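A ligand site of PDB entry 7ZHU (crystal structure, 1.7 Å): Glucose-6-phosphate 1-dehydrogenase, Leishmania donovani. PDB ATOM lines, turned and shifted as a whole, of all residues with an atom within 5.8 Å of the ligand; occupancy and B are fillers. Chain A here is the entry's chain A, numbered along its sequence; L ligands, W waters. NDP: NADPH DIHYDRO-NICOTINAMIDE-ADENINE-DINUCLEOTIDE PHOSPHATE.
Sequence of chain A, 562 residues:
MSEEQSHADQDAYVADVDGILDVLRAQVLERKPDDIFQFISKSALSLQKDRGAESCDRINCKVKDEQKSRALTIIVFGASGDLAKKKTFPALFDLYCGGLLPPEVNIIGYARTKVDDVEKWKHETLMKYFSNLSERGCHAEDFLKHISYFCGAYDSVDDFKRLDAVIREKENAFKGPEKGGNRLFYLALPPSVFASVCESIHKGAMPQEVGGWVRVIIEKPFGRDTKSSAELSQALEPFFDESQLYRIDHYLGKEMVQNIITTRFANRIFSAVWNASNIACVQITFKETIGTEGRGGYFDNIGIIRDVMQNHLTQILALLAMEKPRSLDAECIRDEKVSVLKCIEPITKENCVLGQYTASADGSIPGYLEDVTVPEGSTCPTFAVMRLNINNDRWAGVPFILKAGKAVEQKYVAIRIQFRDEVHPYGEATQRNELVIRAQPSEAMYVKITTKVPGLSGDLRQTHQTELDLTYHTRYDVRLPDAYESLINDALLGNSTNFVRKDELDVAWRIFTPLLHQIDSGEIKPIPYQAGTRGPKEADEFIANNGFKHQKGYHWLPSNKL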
ATOM      1  N   GLY A  78      26.056  11.486  30.125  1.00  0.00           N
ATOM      2  CA  GLY A  78      27.487  11.668  30.242  1.00  0.00           C
ATOM      3  C   GLY A  78      28.051  11.202  31.564  1.00  0.00           C
ATOM      4  O   GLY A  78      29.052  11.736  32.038  1.00  0.00           O
ATOM      5  N   ALA A  79      27.419  10.194  32.175  1.00  0.00           N
ATOM      6  CA  ALA A  79      27.834   9.746  33.504  1.00  0.00           C
ATOM      7  C   ALA A  79      29.240   9.183  33.539  1.00  0.00           C
ATOM      8  O   ALA A  79      29.808   9.026  34.625  1.00  0.00           O
ATOM      9  CB  ALA A  79      26.841   8.697  34.015  1.00  0.00           C
ATOM     10  N   SER A  80      29.811   8.859  32.369  1.00  0.00           N
ATOM     11  CA  SER A  80      31.190   8.373  32.275  1.00  0.00           C
ATOM     12  C   SER A  80      32.216   9.471  32.457  1.00  0.00           C
ATOM     13  O   SER A  80      33.408   9.168  32.508  1.00  0.00           O
ATOM     14  CB  SER A  80      31.401   7.738  30.908  1.00  0.00           C
ATOM     15  OG  SER A  80      31.166   8.702  29.894  1.00  0.00           O
ATOM     16  N   GLY A  81      31.791  10.732  32.577  1.00  0.00           N
ATOM     17  CA  GLY A  81      32.664  11.866  32.380  1.00  0.00           C
ATOM     18  C   GLY A  81      33.256  12.465  33.644  1.00  0.00           C
ATOM     19  O   GLY A  81      32.970  12.057  34.774  1.00  0.00           O
ATOM     20  N   ASP A  82      34.097  13.484  33.431  1.00  0.00           N
ATOM     21  CA  ASP A  82      34.823  14.132  34.508  1.00  0.00           C
ATOM     22  C   ASP A  82      33.893  14.862  35.470  1.00  0.00           C
ATOM     23  O   ASP A  82      34.006  14.727  36.691  1.00  0.00           O
ATOM     24  CB  ASP A  82      35.851  15.104  33.923  1.00  0.00           C
ATOM     25  CG  ASP A  82      36.756  15.709  34.977  1.00  0.00           C
ATOM     26  OD1 ASP A  82      36.341  16.671  35.651  1.00  0.00           O
ATOM     27  OD2 ASP A  82      37.886  15.193  35.140  1.00  0.00           O
ATOM     28  N   LEU A  83      32.965  15.668  34.932  1.00  0.00           N
ATOM     29  CA  LEU A  83      32.037  16.388  35.798  1.00  0.00           C
ATOM     30  C   LEU A  83      31.163  15.428  36.602  1.00  0.00           C
ATOM     31  O   LEU A  83      31.013  15.578  37.821  1.00  0.00           O
ATOM     32  CB  LEU A  83      31.157  17.327  34.982  1.00  0.00           C
ATOM     33  CG  LEU A  83      30.134  18.067  35.876  1.00  0.00           C
ATOM     34  CD1 LEU A  83      30.814  19.140  36.722  1.00  0.00           C
ATOM     35  CD2 LEU A  83      28.991  18.661  35.064  1.00  0.00           C
ATOM     36  N   ALA A  84      30.558  14.445  35.916  1.00  0.00           N
ATOM     37  CA  ALA A  84      29.655  13.532  36.612  1.00  0.00           C
ATOM     38  C   ALA A  84      30.344  12.858  37.794  1.00  0.00           C
ATOM     39  O   ALA A  84      29.854  12.920  38.922  1.00  0.00           O
ATOM     40  CB  ALA A  84      29.110  12.487  35.627  1.00  0.00           C
ATOM     41  N   LYS A  87      31.919  15.743  40.446  1.00  0.00           N
ATOM     42  CA  LYS A  87      31.094  16.791  41.014  1.00  0.00           C
ATOM     43  C   LYS A  87      29.622  16.412  41.101  1.00  0.00           C
ATOM     44  O   LYS A  87      29.008  16.605  42.154  1.00  0.00           O
ATOM     45  CB  LYS A  87      31.287  18.075  40.199  1.00  0.00           C
ATOM     46  CG  LYS A  87      32.664  18.759  40.424  1.00  0.00           C
ATOM     47  CD  LYS A  87      32.814  20.019  39.571  1.00  0.00           C
ATOM     48  CE  LYS A  87      34.203  20.666  39.725  1.00  0.00           C
ATOM     49  NZ  LYS A  87      34.437  21.737  38.690  1.00  0.00           N
ATOM     50  N   ALA A 111      25.304   6.803  29.341  1.00  0.00           N
ATOM     51  CA  ALA A 111      26.471   7.214  28.590  1.00  0.00           C
ATOM     52  C   ALA A 111      26.725   6.184  27.504  1.00  0.00           C
ATOM     53  O   ALA A 111      26.161   5.090  27.515  1.00  0.00           O
ATOM     54  CB  ALA A 111      27.702   7.381  29.491  1.00  0.00           C
ATOM     55  N   ARG A 112      27.563   6.548  26.535  1.00  0.00           N
ATOM     56  CA  ARG A 112      27.907   5.631  25.458  1.00  0.00           C
ATOM     57  C   ARG A 112      28.904   4.579  25.902  1.00  0.00           C
ATOM     58  O   ARG A 112      28.988   3.518  25.271  1.00  0.00           O
ATOM     59  CB  ARG A 112      28.494   6.391  24.270  1.00  0.00           C
ATOM     60  CG  ARG A 112      27.529   7.331  23.574  1.00  0.00           C
ATOM     61  CD  ARG A 112      28.296   8.193  22.595  1.00  0.00           C
ATOM     62  NE  ARG A 112      29.472   8.786  23.219  1.00  0.00           N
ATOM     63  CZ  ARG A 112      30.465   9.347  22.555  1.00  0.00           C
ATOM     64  NH1 ARG A 112      30.467   9.372  21.239  1.00  0.00           N
ATOM     65  NH2 ARG A 112      31.470   9.913  23.231  1.00  0.00           N
ATOM     66  N   THR A 113      29.684   4.860  26.946  1.00  0.00           N
ATOM     67  CA  THR A 113      30.734   3.940  27.342  1.00  0.00           C
ATOM     68  C   THR A 113      30.154   2.616  27.790  1.00  0.00           C
ATOM     69  O   THR A 113      29.243   2.577  28.628  1.00  0.00           O
ATOM     70  CB  THR A 113      31.582   4.553  28.470  1.00  0.00           C
ATOM     71  OG1 THR A 113      32.260   5.715  27.966  1.00  0.00           O
ATOM     72  CG2 THR A 113      32.600   3.553  28.990  1.00  0.00           C
ATOM     73  N   TYR A 149      22.922   2.066  35.669  1.00  0.00           N
ATOM     74  CA  TYR A 149      23.655   2.558  34.516  1.00  0.00           C
ATOM     75  C   TYR A 149      23.003   2.011  33.262  1.00  0.00           C
ATOM     76  O   TYR A 149      22.725   0.822  33.162  1.00  0.00           O
ATOM     77  CB  TYR A 149      25.122   2.129  34.601  1.00  0.00           C
ATOM     78  CG  TYR A 149      26.019   2.718  33.538  1.00  0.00           C
ATOM     79  CD1 TYR A 149      26.622   3.957  33.717  1.00  0.00           C
ATOM     80  CD2 TYR A 149      26.281   2.024  32.350  1.00  0.00           C
ATOM     81  CE1 TYR A 149      27.449   4.503  32.751  1.00  0.00           C
ATOM     82  CE2 TYR A 149      27.082   2.570  31.366  1.00  0.00           C
ATOM     83  CZ  TYR A 149      27.676   3.806  31.577  1.00  0.00           C
ATOM     84  OH  TYR A 149      28.500   4.339  30.610  1.00  0.00           O
ATOM     85  N   GLY A 152      23.841   3.665  26.337  1.00  0.00           N
ATOM     86  CA  GLY A 152      23.040   3.982  25.165  1.00  0.00           C
ATOM     87  C   GLY A 152      23.639   5.120  24.366  1.00  0.00           C
ATOM     88  O   GLY A 152      24.644   5.721  24.750  1.00  0.00           O
ATOM     89  N   TYR A 154      23.055   8.944  22.729  1.00  0.00           N
ATOM     90  CA  TYR A 154      22.313  10.179  22.991  1.00  0.00           C
ATOM     91  C   TYR A 154      21.367  10.525  21.851  1.00  0.00           C
ATOM     92  O   TYR A 154      20.398  11.262  22.074  1.00  0.00           O
ATOM     93  CB  TYR A 154      23.298  11.313  23.241  1.00  0.00           C
ATOM     94  CG  TYR A 154      24.314  10.964  24.310  1.00  0.00           C
ATOM     95  CD1 TYR A 154      23.913  10.763  25.626  1.00  0.00           C
ATOM     96  CD2 TYR A 154      25.662  10.849  23.998  1.00  0.00           C
ATOM     97  CE1 TYR A 154      24.826  10.436  26.601  1.00  0.00           C
ATOM     98  CE2 TYR A 154      26.592  10.519  24.971  1.00  0.00           C
ATOM     99  CZ  TYR A 154      26.163  10.304  26.266  1.00  0.00           C
ATOM    100  OH  TYR A 154      27.090   9.990  27.233  1.00  0.00           O
ATOM    101  N   LEU A 187      22.501  17.066  31.967  1.00  0.00           N
ATOM    102  CA  LEU A 187      23.350  16.943  30.758  1.00  0.00           C
ATOM    103  C   LEU A 187      24.791  17.236  31.143  1.00  0.00           C
ATOM    104  O   LEU A 187      25.298  18.345  30.972  1.00  0.00           O
ATOM    105  CB  LEU A 187      22.868  17.875  29.647  1.00  0.00           C
ATOM    106  CG  LEU A 187      21.426  17.688  29.172  1.00  0.00           C
ATOM    107  CD1 LEU A 187      21.210  18.293  27.802  1.00  0.00           C
ATOM    108  CD2 LEU A 187      21.080  16.261  29.157  1.00  0.00           C
ATOM    109  N   ALA A 188      25.472  16.220  31.680  1.00  0.00           N
ATOM    110  CA  ALA A 188      26.892  16.344  31.999  1.00  0.00           C
ATOM    111  C   ALA A 188      27.732  15.972  30.771  1.00  0.00           C
ATOM    112  O   ALA A 188      28.561  15.082  30.817  1.00  0.00           O
ATOM    113  CB  ALA A 188      27.240  15.481  33.209  1.00  0.00           C
ATOM    114  N   LEU A 189      27.494  16.699  29.686  1.00  0.00           N
ATOM    115  CA  LEU A 189      27.994  16.406  28.359  1.00  0.00           C
ATOM    116  C   LEU A 189      28.469  17.687  27.697  1.00  0.00           C
ATOM    117  O   LEU A 189      28.074  18.786  28.103  1.00  0.00           O
ATOM    118  CB  LEU A 189      26.896  15.801  27.473  1.00  0.00           C
ATOM    119  CG  LEU A 189      26.206  14.519  27.851  1.00  0.00           C
ATOM    120  CD1 LEU A 189      24.767  14.600  27.365  1.00  0.00           C
ATOM    121  CD2 LEU A 189      26.922  13.405  27.157  1.00  0.00           C
ATOM    122  N   PRO A 190      29.269  17.591  26.638  1.00  0.00           N
ATOM    123  CA  PRO A 190      29.587  18.780  25.829  1.00  0.00           C
ATOM    124  C   PRO A 190      28.309  19.370  25.255  1.00  0.00           C
ATOM    125  O   PRO A 190      27.380  18.623  24.889  1.00  0.00           O
ATOM    126  CB  PRO A 190      30.491  18.239  24.716  1.00  0.00           C
ATOM    127  CG  PRO A 190      30.982  16.916  25.207  1.00  0.00           C
ATOM    128  CD  PRO A 190      29.903  16.372  26.100  1.00  0.00           C
ATOM    129  N   PRO A 191      28.201  20.694  25.162  1.00  0.00           N
ATOM    130  CA  PRO A 191      26.968  21.293  24.632  1.00  0.00           C
ATOM    131  C   PRO A 191      26.669  20.909  23.190  1.00  0.00           C
ATOM    132  O   PRO A 191      25.517  21.025  22.771  1.00  0.00           O
ATOM    133  CB  PRO A 191      27.221  22.799  24.782  1.00  0.00           C
ATOM    134  CG  PRO A 191      28.205  22.898  25.902  1.00  0.00           C
ATOM    135  CD  PRO A 191      29.102  21.702  25.748  1.00  0.00           C
ATOM    136  N   SER A 192      27.671  20.438  22.435  1.00  0.00           N
ATOM    137  CA  SER A 192      27.430  19.939  21.086  1.00  0.00           C
ATOM    138  C   SER A 192      26.476  18.745  21.056  1.00  0.00           C
ATOM    139  O   SER A 192      25.977  18.404  19.981  1.00  0.00           O
ATOM    140  CB  SER A 192      28.744  19.539  20.425  1.00  0.00           C
ATOM    141  OG  SER A 192      29.379  18.483  21.132  1.00  0.00           O
ATOM    142  N   VAL A 193      26.255  18.092  22.201  1.00  0.00           N
ATOM    143  CA  VAL A 193      25.344  16.955  22.296  1.00  0.00           C
ATOM    144  C   VAL A 193      23.960  17.345  22.840  1.00  0.00           C
ATOM    145  O   VAL A 193      23.045  16.510  22.833  1.00  0.00           O
ATOM    146  CB  VAL A 193      25.971  15.845  23.165  1.00  0.00           C
ATOM    147  CG1 VAL A 193      25.217  14.518  23.046  1.00  0.00           C
ATOM    148  CG2 VAL A 193      27.428  15.640  22.781  1.00  0.00           C
ATOM    149  N   PHE A 194      23.771  18.597  23.291  1.00  0.00           N
ATOM    150  CA  PHE A 194      22.547  18.953  24.011  1.00  0.00           C
ATOM    151  C   PHE A 194      21.307  18.791  23.132  1.00  0.00           C
ATOM    152  O   PHE A 194      20.301  18.224  23.569  1.00  0.00           O
ATOM    153  CB  PHE A 194      22.612  20.389  24.542  1.00  0.00           C
ATOM    154  CG  PHE A 194      23.583  20.575  25.682  1.00  0.00           C
ATOM    155  CD1 PHE A 194      24.205  19.489  26.287  1.00  0.00           C
ATOM    156  CD2 PHE A 194      23.865  21.864  26.157  1.00  0.00           C
ATOM    157  CE1 PHE A 194      25.085  19.666  27.328  1.00  0.00           C
ATOM    158  CE2 PHE A 194      24.753  22.052  27.207  1.00  0.00           C
ATOM    159  CZ  PHE A 194      25.365  20.950  27.790  1.00  0.00           C
ATOM    160  N   GLU A 219      24.464  22.373  31.041  1.00  0.00           N
ATOM    161  CA  GLU A 219      25.779  22.832  31.491  1.00  0.00           C
ATOM    162  C   GLU A 219      26.345  23.877  30.551  1.00  0.00           C
ATOM    163  O   GLU A 219      25.999  23.934  29.366  1.00  0.00           O
ATOM    164  CB  GLU A 219      26.759  21.664  31.592  1.00  0.00           C
ATOM    165  CG  GLU A 219      26.646  20.879  32.891  1.00  0.00           C
ATOM    166  CD  GLU A 219      27.132  21.686  34.084  1.00  0.00           C
ATOM    167  OE1 GLU A 219      27.799  22.723  33.858  1.00  0.00           O
ATOM    168  OE2 GLU A 219      26.878  21.285  35.230  1.00  0.00           O
ATOM    169  N   LYS A 220      27.222  24.728  31.089  1.00  0.00           N
ATOM    170  CA  LYS A 220      27.949  25.685  30.285  1.00  0.00           C
ATOM    171  C   LYS A 220      29.029  24.976  29.470  1.00  0.00           C
ATOM    172  O   LYS A 220      29.457  23.869  29.819  1.00  0.00           O
ATOM    173  CB  LYS A 220      28.572  26.750  31.173  1.00  0.00           C
ATOM    174  CG  LYS A 220      29.801  26.278  31.922  1.00  0.00           C
ATOM    175  CD  LYS A 220      30.279  27.398  32.863  1.00  0.00           C
ATOM    176  CE  LYS A 220      31.566  27.017  33.550  1.00  0.00           C
ATOM    177  NZ  LYS A 220      32.702  27.087  32.605  1.00  0.00           N
ATOM    178  N   PRO A 221      29.522  25.590  28.371  1.00  0.00           N
ATOM    179  CA  PRO A 221      29.160  26.904  27.825  1.00  0.00           C
ATOM    180  C   PRO A 221      27.848  26.959  27.061  1.00  0.00           C
ATOM    181  O   PRO A 221      27.522  26.094  26.247  1.00  0.00           O
ATOM    182  CB  PRO A 221      30.345  27.224  26.893  1.00  0.00           C
ATOM    183  CG  PRO A 221      30.854  25.870  26.460  1.00  0.00           C
ATOM    184  CD  PRO A 221      30.662  24.974  27.663  1.00  0.00           C
ATOM    185  N   HIS A 250      27.440  26.967  38.610  1.00  0.00           N
ATOM    186  CA  HIS A 250      27.786  26.281  39.855  1.00  0.00           C
ATOM    187  C   HIS A 250      28.167  27.240  40.963  1.00  0.00           C
ATOM    188  O   HIS A 250      28.096  26.867  42.139  1.00  0.00           O
ATOM    189  CB  HIS A 250      28.951  25.305  39.648  1.00  0.00           C
ATOM    190  CG  HIS A 250      28.645  24.142  38.754  1.00  0.00           C
ATOM    191  ND1 HIS A 250      29.352  22.969  38.811  1.00  0.00           N
ATOM    192  CD2 HIS A 250      27.726  23.979  37.775  1.00  0.00           C
ATOM    193  CE1 HIS A 250      28.900  22.130  37.897  1.00  0.00           C
ATOM    194  NE2 HIS A 250      27.909  22.722  37.249  1.00  0.00           N
HETATM  195  PA  NDP L   1      33.512  15.525  28.964  1.00  0.00           P
HETATM  196  O1A NDP L   1      34.161  15.959  27.693  1.00  0.00           O
HETATM  197  O2A NDP L   1      34.425  14.710  29.785  1.00  0.00           O
HETATM  198  O5B NDP L   1      32.134  14.655  28.600  1.00  0.00           O
HETATM  199  C5B NDP L   1      31.558  13.872  29.603  1.00  0.00           C
HETATM  200  C4B NDP L   1      31.026  12.633  28.897  1.00  0.00           C
HETATM  201  O4B NDP L   1      30.348  12.999  27.849  1.00  0.00           O
HETATM  202  C3B NDP L   1      32.238  11.864  28.327  1.00  0.00           C
HETATM  203  O3B NDP L   1      32.668  10.966  29.293  1.00  0.00           O
HETATM  204  C2B NDP L   1      31.607  11.151  27.170  1.00  0.00           C
HETATM  205  O2B NDP L   1      30.869  10.011  27.766  1.00  0.00           O
HETATM  206  C1B NDP L   1      30.707  12.006  26.663  1.00  0.00           C
HETATM  207  N9A NDP L   1      31.320  12.788  25.615  1.00  0.00           N
HETATM  208  C8A NDP L   1      32.399  13.557  25.447  1.00  0.00           C
HETATM  209  N7A NDP L   1      32.393  14.004  24.182  1.00  0.00           N
HETATM  210  C5A NDP L   1      31.305  13.502  23.576  1.00  0.00           C
HETATM  211  C6A NDP L   1      30.834  13.664  22.296  1.00  0.00           C
HETATM  212  N6A NDP L   1      31.319  14.394  21.143  1.00  0.00           N
HETATM  213  N1A NDP L   1      29.699  13.057  21.911  1.00  0.00           N
HETATM  214  C2A NDP L   1      29.017  12.291  22.807  1.00  0.00           C
HETATM  215  N3A NDP L   1      29.482  12.131  24.080  1.00  0.00           N
HETATM  216  C4A NDP L   1      30.631  12.750  24.458  1.00  0.00           C
HETATM  217  O3  NDP L   1      33.018  16.870  29.762  1.00  0.00           O
HETATM  218  PN  NDP L   1      33.010  17.147  31.409  1.00  0.00           P
HETATM  219  O1N NDP L   1      32.698  15.929  32.206  1.00  0.00           O
HETATM  220  O2N NDP L   1      34.317  17.713  31.817  1.00  0.00           O
HETATM  221  O5D NDP L   1      31.831  18.248  31.621  1.00  0.00           O
HETATM  222  C5D NDP L   1      30.489  17.890  31.217  1.00  0.00           C
HETATM  223  C4D NDP L   1      29.768  19.285  31.007  1.00  0.00           C
HETATM  224  O4D NDP L   1      29.963  19.993  32.068  1.00  0.00           O
HETATM  225  C3D NDP L   1      30.400  20.083  29.858  1.00  0.00           C
HETATM  226  O3D NDP L   1      29.367  20.777  29.205  1.00  0.00           O
HETATM  227  C2D NDP L   1      31.312  21.076  30.549  1.00  0.00           C
HETATM  228  O2D NDP L   1      31.478  22.301  29.662  1.00  0.00           O
HETATM  229  C1D NDP L   1      30.628  21.367  31.618  1.00  0.00           C
HETATM  230  N1N NDP L   1      31.448  21.765  32.777  1.00  0.00           N
HETATM  231  C2N NDP L   1      32.588  20.997  33.167  1.00  0.00           C
HETATM  232  C3N NDP L   1      33.189  21.157  34.518  1.00  0.00           C
HETATM  233  C7N NDP L   1      34.084  20.055  35.044  1.00  0.00           C
HETATM  234  O7N NDP L   1      34.330  19.073  34.356  1.00  0.00           O
HETATM  235  N7N NDP L   1      34.660  20.162  36.337  1.00  0.00           N
HETATM  236  C4N NDP L   1      32.570  22.161  35.576  1.00  0.00           C
HETATM  237  C5N NDP L   1      31.221  22.811  35.088  1.00  0.00           C
HETATM  238  C6N NDP L   1      31.029  22.932  33.560  1.00  0.00           C
HETATM  239  P2B NDP L   1      30.551   8.708  26.793  1.00  0.00           P
HETATM  240  O1X NDP L   1      30.544   7.564  27.731  1.00  0.00           O
HETATM  241  O2X NDP L   1      29.188   8.869  26.123  1.00  0.00           O
HETATM  242  O3X NDP L   1      31.596   8.561  25.734  1.00  0.00           O
HETATM  243  O   HOH W   1      32.380  21.404  26.796  1.00  0.00           O
HETATM  244  O   HOH W   2      34.168   8.512  26.157  1.00  0.00           O
HETATM  245  O   HOH W   3      29.749  16.319  19.070  1.00  0.00           O
HETATM  246  O   HOH W   4      35.328  18.076  37.574  1.00  0.00           O
HETATM  247  O   HOH W   5      34.872  20.132  30.340  1.00  0.00           O
HETATM  248  O   HOH W   6      34.477  11.199  25.470  1.00  0.00           O
HETATM  249  O   HOH W   7      37.189  17.324  31.610  1.00  0.00           O
HETATM  250  O   HOH W   8      30.640  14.266  32.966  1.00  0.00           O
HETATM  251  O   HOH W   9      31.249  25.208  36.787  1.00  0.00           O
HETATM  252  O   HOH W  10      28.432  13.062  19.122  1.00  0.00           O
HETATM  253  O   HOH W  11      32.133   6.009  24.326  1.00  0.00           O
HETATM  254  O   HOH W  12      33.760  19.394  27.665  1.00  0.00           O
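The side-chain hydroxyl of Ser 80 lies within hydrogen-bond range of an oxygen (O2B) of the ligand (2.5 Å).
The backbone NH of Thr 113 sits at hydrogen-bond distance from an oxygen (O1X) of the ligand (2.9 Å).
The side-chain hydroxyl (OG1) of Thr 113 is in hydrogen-bond range of an oxygen (O1X) of the ligand (2.5 Å).
An oxygen (O2D) of the ligand lies within hydrogen-bond range of the backbone carbonyl oxygen (O) of Lys 220, 2.6 Å away.
O of Leu 189 lies within hydrogen-bond range of O3D of the ligand (2.6 Å).
The side-chain hydroxyl (OH) of Tyr 154 lies within hydrogen-bond range of an oxygen (O2X) of the ligand (2.6 Å).
An oxygen (O1N) of the ligand lies within hydrogen-bond range of the backbone NH (N) of Leu 83.
N of Arg 112 lies within hydrogen-bond range of O2X of the ligand, at 2.9 Å.
An oxygen (O3X) of the ligand lies within salt-bridge range of the guanidinium group (NH2) of Arg 112, at 2.8 Å.
The backbone NH (N) of Asp 82 is in hydrogen-bond range of an oxygen (O1N) of the ligand (3.1 Å).
N of Gly 81 sits close to O3B of the ligand (3.4 Å).
OH of Tyr 149 lies within hydrogen-bond range of O of Thr 113.
The side-chain hydroxyl (OH) of Tyr 154 is in hydrogen-bond range of the backbone NH (N) of Gly 78, at 3.4 Å.
NE2 of His 250 sits at hydrogen-bond distance from OE2 of Glu 219 (2.7 Å).
O of Ala 111 lies within hydrogen-bond range of N of Gly 152.
A nitrogen (N7N) of the ligand sits close to the side-chain amino group of Lys 87 (2.8 Å).
Merely in contact with the ligand: Gly 78, Ala 111, Ala 188, Pro 190, Pro 191, Val 193, Glu 219, Pro 221 and His 250.
Hydrophobic or aromatic side chains that line the ligand: Leu 83, Ala 111, Tyr 154, Leu 189, Pro 190, Pro 191, Val 193, Pro 221 and His 250.
Within 4 Å of the ligand: Gly 78, Ser 80, Gly 81, Asp 82, Leu 83, Lys 87, Ala 111, Arg 112, Thr 113, Tyr 154, Ala 188, Leu 189, Pro 190, Pro 191, Val 193, Glu 219, Lys 220, Pro 221 and His 250.
Water W4 lies within hydrogen-bond range of a nitrogen (N7N) of the ligand (2.5 Å) and the side-chain carboxylate (OD1) of Asp 82 (2.6 Å).
Water W8 lies within hydrogen-bond range of O1N of the ligand (2.8 Å), N of Ala 84 (3.0 Å), O of Ala 188 (3.1 Å), O of Gly 78 (3.1 Å) and N of Leu 83 (3.4 Å).
Water W3 lies within hydrogen-bond range of OG of Ser 192 (3.0 Å) and N6A of the ligand (3.2 Å).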
